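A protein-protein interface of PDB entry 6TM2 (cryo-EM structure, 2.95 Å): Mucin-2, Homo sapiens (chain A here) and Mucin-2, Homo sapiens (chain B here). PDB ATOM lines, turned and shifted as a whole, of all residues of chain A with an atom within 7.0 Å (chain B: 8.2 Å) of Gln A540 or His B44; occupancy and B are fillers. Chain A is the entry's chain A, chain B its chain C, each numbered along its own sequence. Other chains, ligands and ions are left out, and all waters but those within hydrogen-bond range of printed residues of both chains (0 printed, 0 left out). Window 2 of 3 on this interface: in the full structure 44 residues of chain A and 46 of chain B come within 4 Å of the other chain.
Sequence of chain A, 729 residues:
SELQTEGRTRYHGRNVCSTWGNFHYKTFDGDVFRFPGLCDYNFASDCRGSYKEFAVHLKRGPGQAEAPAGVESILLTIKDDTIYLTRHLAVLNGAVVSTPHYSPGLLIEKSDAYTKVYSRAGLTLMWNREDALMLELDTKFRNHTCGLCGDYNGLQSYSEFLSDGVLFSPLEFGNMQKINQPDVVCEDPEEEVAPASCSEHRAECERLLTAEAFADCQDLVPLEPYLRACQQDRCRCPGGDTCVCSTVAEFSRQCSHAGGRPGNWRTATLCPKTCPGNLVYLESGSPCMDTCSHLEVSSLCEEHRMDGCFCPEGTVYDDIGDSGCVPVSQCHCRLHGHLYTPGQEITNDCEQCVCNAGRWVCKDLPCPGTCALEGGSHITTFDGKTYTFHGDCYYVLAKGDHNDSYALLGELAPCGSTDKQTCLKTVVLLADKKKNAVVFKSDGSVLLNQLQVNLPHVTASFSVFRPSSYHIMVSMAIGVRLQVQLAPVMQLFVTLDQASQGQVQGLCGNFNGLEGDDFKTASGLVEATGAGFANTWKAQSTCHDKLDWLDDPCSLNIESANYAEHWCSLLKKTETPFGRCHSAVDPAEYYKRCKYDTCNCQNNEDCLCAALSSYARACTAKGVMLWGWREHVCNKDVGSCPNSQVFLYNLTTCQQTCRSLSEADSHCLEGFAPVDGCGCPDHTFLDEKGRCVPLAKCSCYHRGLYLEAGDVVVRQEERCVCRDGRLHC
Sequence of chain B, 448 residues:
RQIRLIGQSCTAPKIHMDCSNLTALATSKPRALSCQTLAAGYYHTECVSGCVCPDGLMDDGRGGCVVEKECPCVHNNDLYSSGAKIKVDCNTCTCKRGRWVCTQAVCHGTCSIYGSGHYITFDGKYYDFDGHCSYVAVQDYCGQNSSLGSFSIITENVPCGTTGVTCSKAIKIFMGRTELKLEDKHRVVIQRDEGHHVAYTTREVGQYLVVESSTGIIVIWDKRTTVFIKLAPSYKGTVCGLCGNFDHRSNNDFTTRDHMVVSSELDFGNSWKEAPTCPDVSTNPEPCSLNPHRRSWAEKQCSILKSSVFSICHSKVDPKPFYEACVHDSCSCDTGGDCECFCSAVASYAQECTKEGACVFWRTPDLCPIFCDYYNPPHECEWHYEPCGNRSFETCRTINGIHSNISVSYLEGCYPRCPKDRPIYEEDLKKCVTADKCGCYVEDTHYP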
ATOM      1  N   ASP A 392      20.065 -16.108 -22.030  1.00  0.00           N
ATOM      2  CA  ASP A 392      21.382 -15.470 -21.888  1.00  0.00           C
ATOM      3  C   ASP A 392      21.916 -15.784 -20.487  1.00  0.00           C
ATOM      4  O   ASP A 392      21.837 -14.925 -19.606  1.00  0.00           O
ATOM      5  CB  ASP A 392      21.266 -13.968 -22.113  1.00  0.00           C
ATOM      6  CG  ASP A 392      22.607 -13.248 -22.175  1.00  0.00           C
ATOM      7  OD1 ASP A 392      23.676 -13.868 -22.030  1.00  0.00           O
ATOM      8  OD2 ASP A 392      22.584 -12.020 -22.379  1.00  0.00           O
ATOM      9  N   CYS A 393      22.570 -16.950 -20.340  1.00  0.00           N
ATOM     10  CA  CYS A 393      23.151 -17.414 -19.074  1.00  0.00           C
ATOM     11  C   CYS A 393      23.837 -18.767 -19.270  1.00  0.00           C
ATOM     12  O   CYS A 393      23.840 -19.302 -20.378  1.00  0.00           O
ATOM     13  CB  CYS A 393      22.082 -17.552 -17.977  1.00  0.00           C
ATOM     14  SG  CYS A 393      22.698 -17.707 -16.312  1.00  0.00           S
ATOM     15  N   TYR A 394      24.420 -19.327 -18.210  1.00  0.00           N
ATOM     16  CA  TYR A 394      24.676 -20.762 -18.115  1.00  0.00           C
ATOM     17  C   TYR A 394      23.437 -21.469 -17.589  1.00  0.00           C
ATOM     18  O   TYR A 394      22.812 -21.006 -16.633  1.00  0.00           O
ATOM     19  CB  TYR A 394      25.847 -21.075 -17.180  1.00  0.00           C
ATOM     20  CG  TYR A 394      27.238 -20.818 -17.704  1.00  0.00           C
ATOM     21  CD1 TYR A 394      27.476 -20.653 -19.050  1.00  0.00           C
ATOM     22  CD2 TYR A 394      28.322 -20.767 -16.841  1.00  0.00           C
ATOM     23  CE1 TYR A 394      28.745 -20.431 -19.528  1.00  0.00           C
ATOM     24  CE2 TYR A 394      29.605 -20.542 -17.317  1.00  0.00           C
ATOM     25  CZ  TYR A 394      29.799 -20.374 -18.674  1.00  0.00           C
ATOM     26  OH  TYR A 394      31.049 -20.148 -19.195  1.00  0.00           O
ATOM     27  N   TYR A 395      23.097 -22.604 -18.193  1.00  0.00           N
ATOM     28  CA  TYR A 395      21.888 -23.337 -17.847  1.00  0.00           C
ATOM     29  C   TYR A 395      22.204 -24.799 -17.588  1.00  0.00           C
ATOM     30  O   TYR A 395      23.077 -25.376 -18.234  1.00  0.00           O
ATOM     31  CB  TYR A 395      20.842 -23.230 -18.946  1.00  0.00           C
ATOM     32  CG  TYR A 395      20.255 -21.852 -19.099  1.00  0.00           C
ATOM     33  CD1 TYR A 395      19.231 -21.426 -18.276  1.00  0.00           C
ATOM     34  CD2 TYR A 395      20.730 -20.978 -20.061  1.00  0.00           C
ATOM     35  CE1 TYR A 395      18.696 -20.176 -18.405  1.00  0.00           C
ATOM     36  CE2 TYR A 395      20.200 -19.722 -20.195  1.00  0.00           C
ATOM     37  CZ  TYR A 395      19.183 -19.329 -19.362  1.00  0.00           C
ATOM     38  OH  TYR A 395      18.642 -18.076 -19.485  1.00  0.00           O
ATOM     39  N   LEU A 409      26.355 -28.510 -18.231  1.00  0.00           N
ATOM     40  CA  LEU A 409      25.930 -27.135 -18.417  1.00  0.00           C
ATOM     41  C   LEU A 409      25.993 -26.776 -19.893  1.00  0.00           C
ATOM     42  O   LEU A 409      26.388 -27.576 -20.737  1.00  0.00           O
ATOM     43  CB  LEU A 409      26.798 -26.176 -17.605  1.00  0.00           C
ATOM     44  CG  LEU A 409      26.823 -26.283 -16.087  1.00  0.00           C
ATOM     45  CD1 LEU A 409      27.808 -25.284 -15.555  1.00  0.00           C
ATOM     46  CD2 LEU A 409      25.467 -26.066 -15.485  1.00  0.00           C
ATOM     47  N   TRP A 537      16.415 -22.885 -14.131  1.00  0.00           N
ATOM     48  CA  TRP A 537      17.627 -23.674 -14.290  1.00  0.00           C
ATOM     49  C   TRP A 537      18.827 -22.824 -14.681  1.00  0.00           C
ATOM     50  O   TRP A 537      19.753 -23.317 -15.319  1.00  0.00           O
ATOM     51  CB  TRP A 537      17.431 -24.791 -15.311  1.00  0.00           C
ATOM     52  CG  TRP A 537      16.527 -25.844 -14.832  1.00  0.00           C
ATOM     53  CD1 TRP A 537      15.237 -26.050 -15.194  1.00  0.00           C
ATOM     54  CD2 TRP A 537      16.821 -26.804 -13.823  1.00  0.00           C
ATOM     55  NE1 TRP A 537      14.715 -27.104 -14.494  1.00  0.00           N
ATOM     56  CE2 TRP A 537      15.672 -27.580 -13.642  1.00  0.00           C
ATOM     57  CE3 TRP A 537      17.951 -27.081 -13.055  1.00  0.00           C
ATOM     58  CZ2 TRP A 537      15.625 -28.626 -12.739  1.00  0.00           C
ATOM     59  CZ3 TRP A 537      17.898 -28.111 -12.157  1.00  0.00           C
ATOM     60  CH2 TRP A 537      16.749 -28.873 -12.005  1.00  0.00           C
ATOM     61  N   LYS A 538      18.821 -21.555 -14.302  1.00  0.00           N
ATOM     62  CA  LYS A 538      19.999 -20.720 -14.451  1.00  0.00           C
ATOM     63  C   LYS A 538      21.083 -21.220 -13.511  1.00  0.00           C
ATOM     64  O   LYS A 538      20.817 -21.507 -12.343  1.00  0.00           O
ATOM     65  CB  LYS A 538      19.657 -19.272 -14.128  1.00  0.00           C
ATOM     66  CG  LYS A 538      18.654 -18.651 -15.051  1.00  0.00           C
ATOM     67  CD  LYS A 538      18.480 -17.189 -14.734  1.00  0.00           C
ATOM     68  CE  LYS A 538      17.726 -17.005 -13.441  1.00  0.00           C
ATOM     69  NZ  LYS A 538      17.425 -15.578 -13.159  1.00  0.00           N
ATOM     70  N   ALA A 539      22.300 -21.343 -14.019  1.00  0.00           N
ATOM     71  CA  ALA A 539      23.427 -21.757 -13.199  1.00  0.00           C
ATOM     72  C   ALA A 539      24.118 -20.581 -12.529  1.00  0.00           C
ATOM     73  O   ALA A 539      25.047 -20.789 -11.744  1.00  0.00           O
ATOM     74  CB  ALA A 539      24.432 -22.540 -14.041  1.00  0.00           C
ATOM     75  N   GLN A 540      23.686 -19.359 -12.819  1.00  0.00           N
ATOM     76  CA  GLN A 540      24.220 -18.152 -12.213  1.00  0.00           C
ATOM     77  C   GLN A 540      23.057 -17.316 -11.702  1.00  0.00           C
ATOM     78  O   GLN A 540      22.040 -17.175 -12.382  1.00  0.00           O
ATOM     79  CB  GLN A 540      25.039 -17.357 -13.218  1.00  0.00           C
ATOM     80  CG  GLN A 540      26.298 -18.056 -13.676  1.00  0.00           C
ATOM     81  CD  GLN A 540      27.025 -17.285 -14.753  1.00  0.00           C
ATOM     82  OE1 GLN A 540      26.545 -16.255 -15.223  1.00  0.00           O
ATOM     83  NE2 GLN A 540      28.185 -17.783 -15.155  1.00  0.00           N
ATOM     84  N   SER A 541      23.209 -16.764 -10.502  1.00  0.00           N
ATOM     85  CA  SER A 541      22.121 -16.016  -9.888  1.00  0.00           C
ATOM     86  C   SER A 541      21.947 -14.626 -10.477  1.00  0.00           C
ATOM     87  O   SER A 541      20.862 -14.050 -10.355  1.00  0.00           O
ATOM     88  CB  SER A 541      22.350 -15.901  -8.384  1.00  0.00           C
ATOM     89  OG  SER A 541      23.493 -15.113  -8.111  1.00  0.00           O
ATOM     90  N   THR A 542      22.977 -14.073 -11.111  1.00  0.00           N
ATOM     91  CA  THR A 542      22.942 -12.707 -11.608  1.00  0.00           C
ATOM     92  C   THR A 542      22.482 -12.617 -13.055  1.00  0.00           C
ATOM     93  O   THR A 542      22.703 -11.587 -13.702  1.00  0.00           O
ATOM     94  CB  THR A 542      24.319 -12.063 -11.466  1.00  0.00           C
ATOM     95  OG1 THR A 542      25.265 -12.780 -12.267  1.00  0.00           O
ATOM     96  CG2 THR A 542      24.767 -12.108 -10.016  1.00  0.00           C
ATOM     97  N   CYS A 543      21.867 -13.667 -13.581  1.00  0.00           N
ATOM     98  CA  CYS A 543      21.341 -13.641 -14.933  1.00  0.00           C
ATOM     99  C   CYS A 543      19.924 -13.085 -14.919  1.00  0.00           C
ATOM    100  O   CYS A 543      19.160 -13.311 -13.979  1.00  0.00           O
ATOM    101  CB  CYS A 543      21.355 -15.045 -15.542  1.00  0.00           C
ATOM    102  SG  CYS A 543      23.008 -15.768 -15.771  1.00  0.00           S
ATOM    103  N   HIS A 544      19.581 -12.336 -15.960  1.00  0.00           N
ATOM    104  CA  HIS A 544      18.237 -11.790 -16.037  1.00  0.00           C
ATOM    105  C   HIS A 544      17.255 -12.859 -16.499  1.00  0.00           C
ATOM    106  O   HIS A 544      17.638 -13.895 -17.043  1.00  0.00           O
ATOM    107  CB  HIS A 544      18.186 -10.588 -16.977  1.00  0.00           C
ATOM    108  CG  HIS A 544      18.976  -9.412 -16.493  1.00  0.00           C
ATOM    109  ND1 HIS A 544      18.554  -8.610 -15.456  1.00  0.00           N
ATOM    110  CD2 HIS A 544      20.160  -8.901 -16.905  1.00  0.00           C
ATOM    111  CE1 HIS A 544      19.446  -7.660 -15.246  1.00  0.00           C
ATOM    112  NE2 HIS A 544      20.430  -7.813 -16.112  1.00  0.00           N
ATOM    113  N   ARG B  31      29.534 -17.088  -3.041  1.00  0.00           N
ATOM    114  CA  ARG B  31      28.285 -17.664  -2.558  1.00  0.00           C
ATOM    115  C   ARG B  31      27.205 -16.595  -2.429  1.00  0.00           C
ATOM    116  O   ARG B  31      27.135 -15.889  -1.424  1.00  0.00           O
ATOM    117  CB  ARG B  31      28.500 -18.359  -1.212  1.00  0.00           C
ATOM    118  N   ALA B  32      26.363 -16.481  -3.457  1.00  0.00           N
ATOM    119  CA  ALA B  32      25.265 -15.515  -3.496  1.00  0.00           C
ATOM    120  C   ALA B  32      24.018 -16.249  -3.975  1.00  0.00           C
ATOM    121  O   ALA B  32      23.762 -16.330  -5.179  1.00  0.00           O
ATOM    122  CB  ALA B  32      25.606 -14.332  -4.395  1.00  0.00           C
ATOM    123  N   SER B  34      19.857 -17.078  -4.361  1.00  0.00           N
ATOM    124  CA  SER B  34      18.870 -16.183  -4.947  1.00  0.00           C
ATOM    125  C   SER B  34      17.416 -16.631  -4.844  1.00  0.00           C
ATOM    126  O   SER B  34      16.570 -16.022  -5.513  1.00  0.00           O
ATOM    127  CB  SER B  34      19.204 -15.947  -6.419  1.00  0.00           C
ATOM    128  OG  SER B  34      18.240 -15.115  -7.036  1.00  0.00           O
ATOM    129  N   GLN B  36      15.891 -18.814  -6.354  1.00  0.00           N
ATOM    130  CA  GLN B  36      15.382 -19.332  -7.613  1.00  0.00           C
ATOM    131  C   GLN B  36      16.413 -20.335  -8.087  1.00  0.00           C
ATOM    132  O   GLN B  36      16.099 -21.296  -8.795  1.00  0.00           O
ATOM    133  CB  GLN B  36      15.171 -18.204  -8.620  1.00  0.00           C
ATOM    134  CG  GLN B  36      14.469 -18.610  -9.896  1.00  0.00           C
ATOM    135  CD  GLN B  36      14.249 -17.436 -10.826  1.00  0.00           C
ATOM    136  OE1 GLN B  36      14.701 -16.327 -10.555  1.00  0.00           O
ATOM    137  NE2 GLN B  36      13.524 -17.667 -11.914  1.00  0.00           N
ATOM    138  N   THR B  37      17.651 -20.111  -7.665  1.00  0.00           N
ATOM    139  CA  THR B  37      18.775 -21.004  -7.912  1.00  0.00           C
ATOM    140  C   THR B  37      19.083 -21.855  -6.693  1.00  0.00           C
ATOM    141  O   THR B  37      20.251 -22.101  -6.380  1.00  0.00           O
ATOM    142  CB  THR B  37      19.997 -20.200  -8.328  1.00  0.00           C
ATOM    143  OG1 THR B  37      20.379 -19.332  -7.257  1.00  0.00           O
ATOM    144  CG2 THR B  37      19.671 -19.361  -9.543  1.00  0.00           C
ATOM    145  N   ALA B  40      19.571 -25.367  -8.430  1.00  0.00           N
ATOM    146  CA  ALA B  40      20.508 -25.366  -9.548  1.00  0.00           C
ATOM    147  C   ALA B  40      21.843 -25.974  -9.135  1.00  0.00           C
ATOM    148  O   ALA B  40      22.258 -27.011  -9.664  1.00  0.00           O
ATOM    149  CB  ALA B  40      20.694 -23.946 -10.084  1.00  0.00           C
ATOM    150  N   GLY B  41      22.520 -25.359  -8.168  1.00  0.00           N
ATOM    151  CA  GLY B  41      23.732 -25.949  -7.636  1.00  0.00           C
ATOM    152  C   GLY B  41      24.850 -24.977  -7.320  1.00  0.00           C
ATOM    153  O   GLY B  41      25.833 -25.370  -6.681  1.00  0.00           O
ATOM    154  N   TYR B  42      24.704 -23.723  -7.764  1.00  0.00           N
ATOM    155  CA  TYR B  42      25.650 -22.624  -7.528  1.00  0.00           C
ATOM    156  C   TYR B  42      27.046 -22.976  -8.052  1.00  0.00           C
ATOM    157  O   TYR B  42      28.007 -23.155  -7.300  1.00  0.00           O
ATOM    158  CB  TYR B  42      25.691 -22.232  -6.044  1.00  0.00           C
ATOM    159  N   TYR B  43      27.126 -23.083  -9.377  1.00  0.00           N
ATOM    160  CA  TYR B  43      28.313 -23.633 -10.021  1.00  0.00           C
ATOM    161  C   TYR B  43      29.392 -22.578 -10.240  1.00  0.00           C
ATOM    162  O   TYR B  43      30.480 -22.665  -9.663  1.00  0.00           O
ATOM    163  CB  TYR B  43      27.933 -24.271 -11.359  1.00  0.00           C
ATOM    164  CG  TYR B  43      26.954 -25.408 -11.228  1.00  0.00           C
ATOM    165  CD1 TYR B  43      27.359 -26.646 -10.771  1.00  0.00           C
ATOM    166  CD2 TYR B  43      25.631 -25.247 -11.598  1.00  0.00           C
ATOM    167  CE1 TYR B  43      26.469 -27.687 -10.656  1.00  0.00           C
ATOM    168  CE2 TYR B  43      24.736 -26.284 -11.493  1.00  0.00           C
ATOM    169  CZ  TYR B  43      25.164 -27.506 -11.021  1.00  0.00           C
ATOM    170  OH  TYR B  43      24.287 -28.554 -10.901  1.00  0.00           O
ATOM    171  N   HIS B  44      29.102 -21.580 -11.066  1.00  0.00           N
ATOM    172  CA  HIS B  44      30.120 -20.632 -11.508  1.00  0.00           C
ATOM    173  C   HIS B  44      30.467 -19.613 -10.431  1.00  0.00           C
ATOM    174  O   HIS B  44      31.641 -19.341 -10.184  1.00  0.00           O
ATOM    175  CB  HIS B  44      29.658 -19.911 -12.777  1.00  0.00           C
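The side-chain hydroxyl of Ser A541 is in hydrogen-bond range of the backbone carbonyl oxygen of Ala B32, 3.2 Å away.
The backbone carbonyl oxygen of Tyr A394 sits at hydrogen-bond distance from the backbone NH of Ala A539 (2.7 Å).
NZ of Lys A538 is in hydrogen-bond range of O of Cys A543 (3.0 Å).
SG of Cys A543 sits close to OE1 of Gln A540 (3.6 Å).
The backbone carbonyl oxygen (O) of Ala B40 lies within hydrogen-bond range of the side-chain hydroxyl (OH) of Tyr B43 (2.8 Å).
SG of Cys A393 forms a disulfide with SG of Cys A543 (2.0 Å).
Leu A409 touches Tyr B43.
Lys A538 touches Gln B36.
CG2 of Thr B37 touches O of Lys A538, at 3.7 Å.
O of Lys A538 touches CB of Ala B40, 3.3 Å away.
CB of Ala A539 touches CD2 of Tyr B43, 3.8 Å away.
Gln A540 touches His B44 (NE2 to CB, 3.5 Å).
Ser B34 touches Ser A541 (CB to CB, 3.7 Å).
Of chain B, only His B44 (3.5 Å) comes within 4 Å of Gln A540.
His B44 touches just one residue of chain A: Gln A540 (3.5 Å).
Ala A539 touches one residue of chain B.
Of the printed residues of chain B, Ser A541 touches Ala B32 and Ser B34.
Printed residues of chain A within 4 Å of Tyr B43: Leu A409 (3.98 Å) and Ala A539 (3.8 Å).
Of the printed residues of chain A, Gln B36 touches Lys A538.
Of the printed residues of chain A, Ala B40 touches Lys A538 (3.3 Å).
Trp A537 touches none of the printed residues of chain B.
The nearest residue of chain B that does not touch Gln A540 is Thr B37 (4.3 Å).
The nearest printed residue of chain A that does not touch Thr B37 is Ser A541 (4.1 Å).
Of the 13 printed residues of chain A, 5 touch a printed residue of chain B.
Hydrophobic or aromatic side chains of chain A within 4 Å of the printed part of chain B: Leu A409 and Ala A539.
Among the printed residues, 8 pairs touch across the chains.
Among the printed residues, no Asp or Glu carboxylate lies within 4 Å of a Lys or Arg side-chain nitrogen of the other chain.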
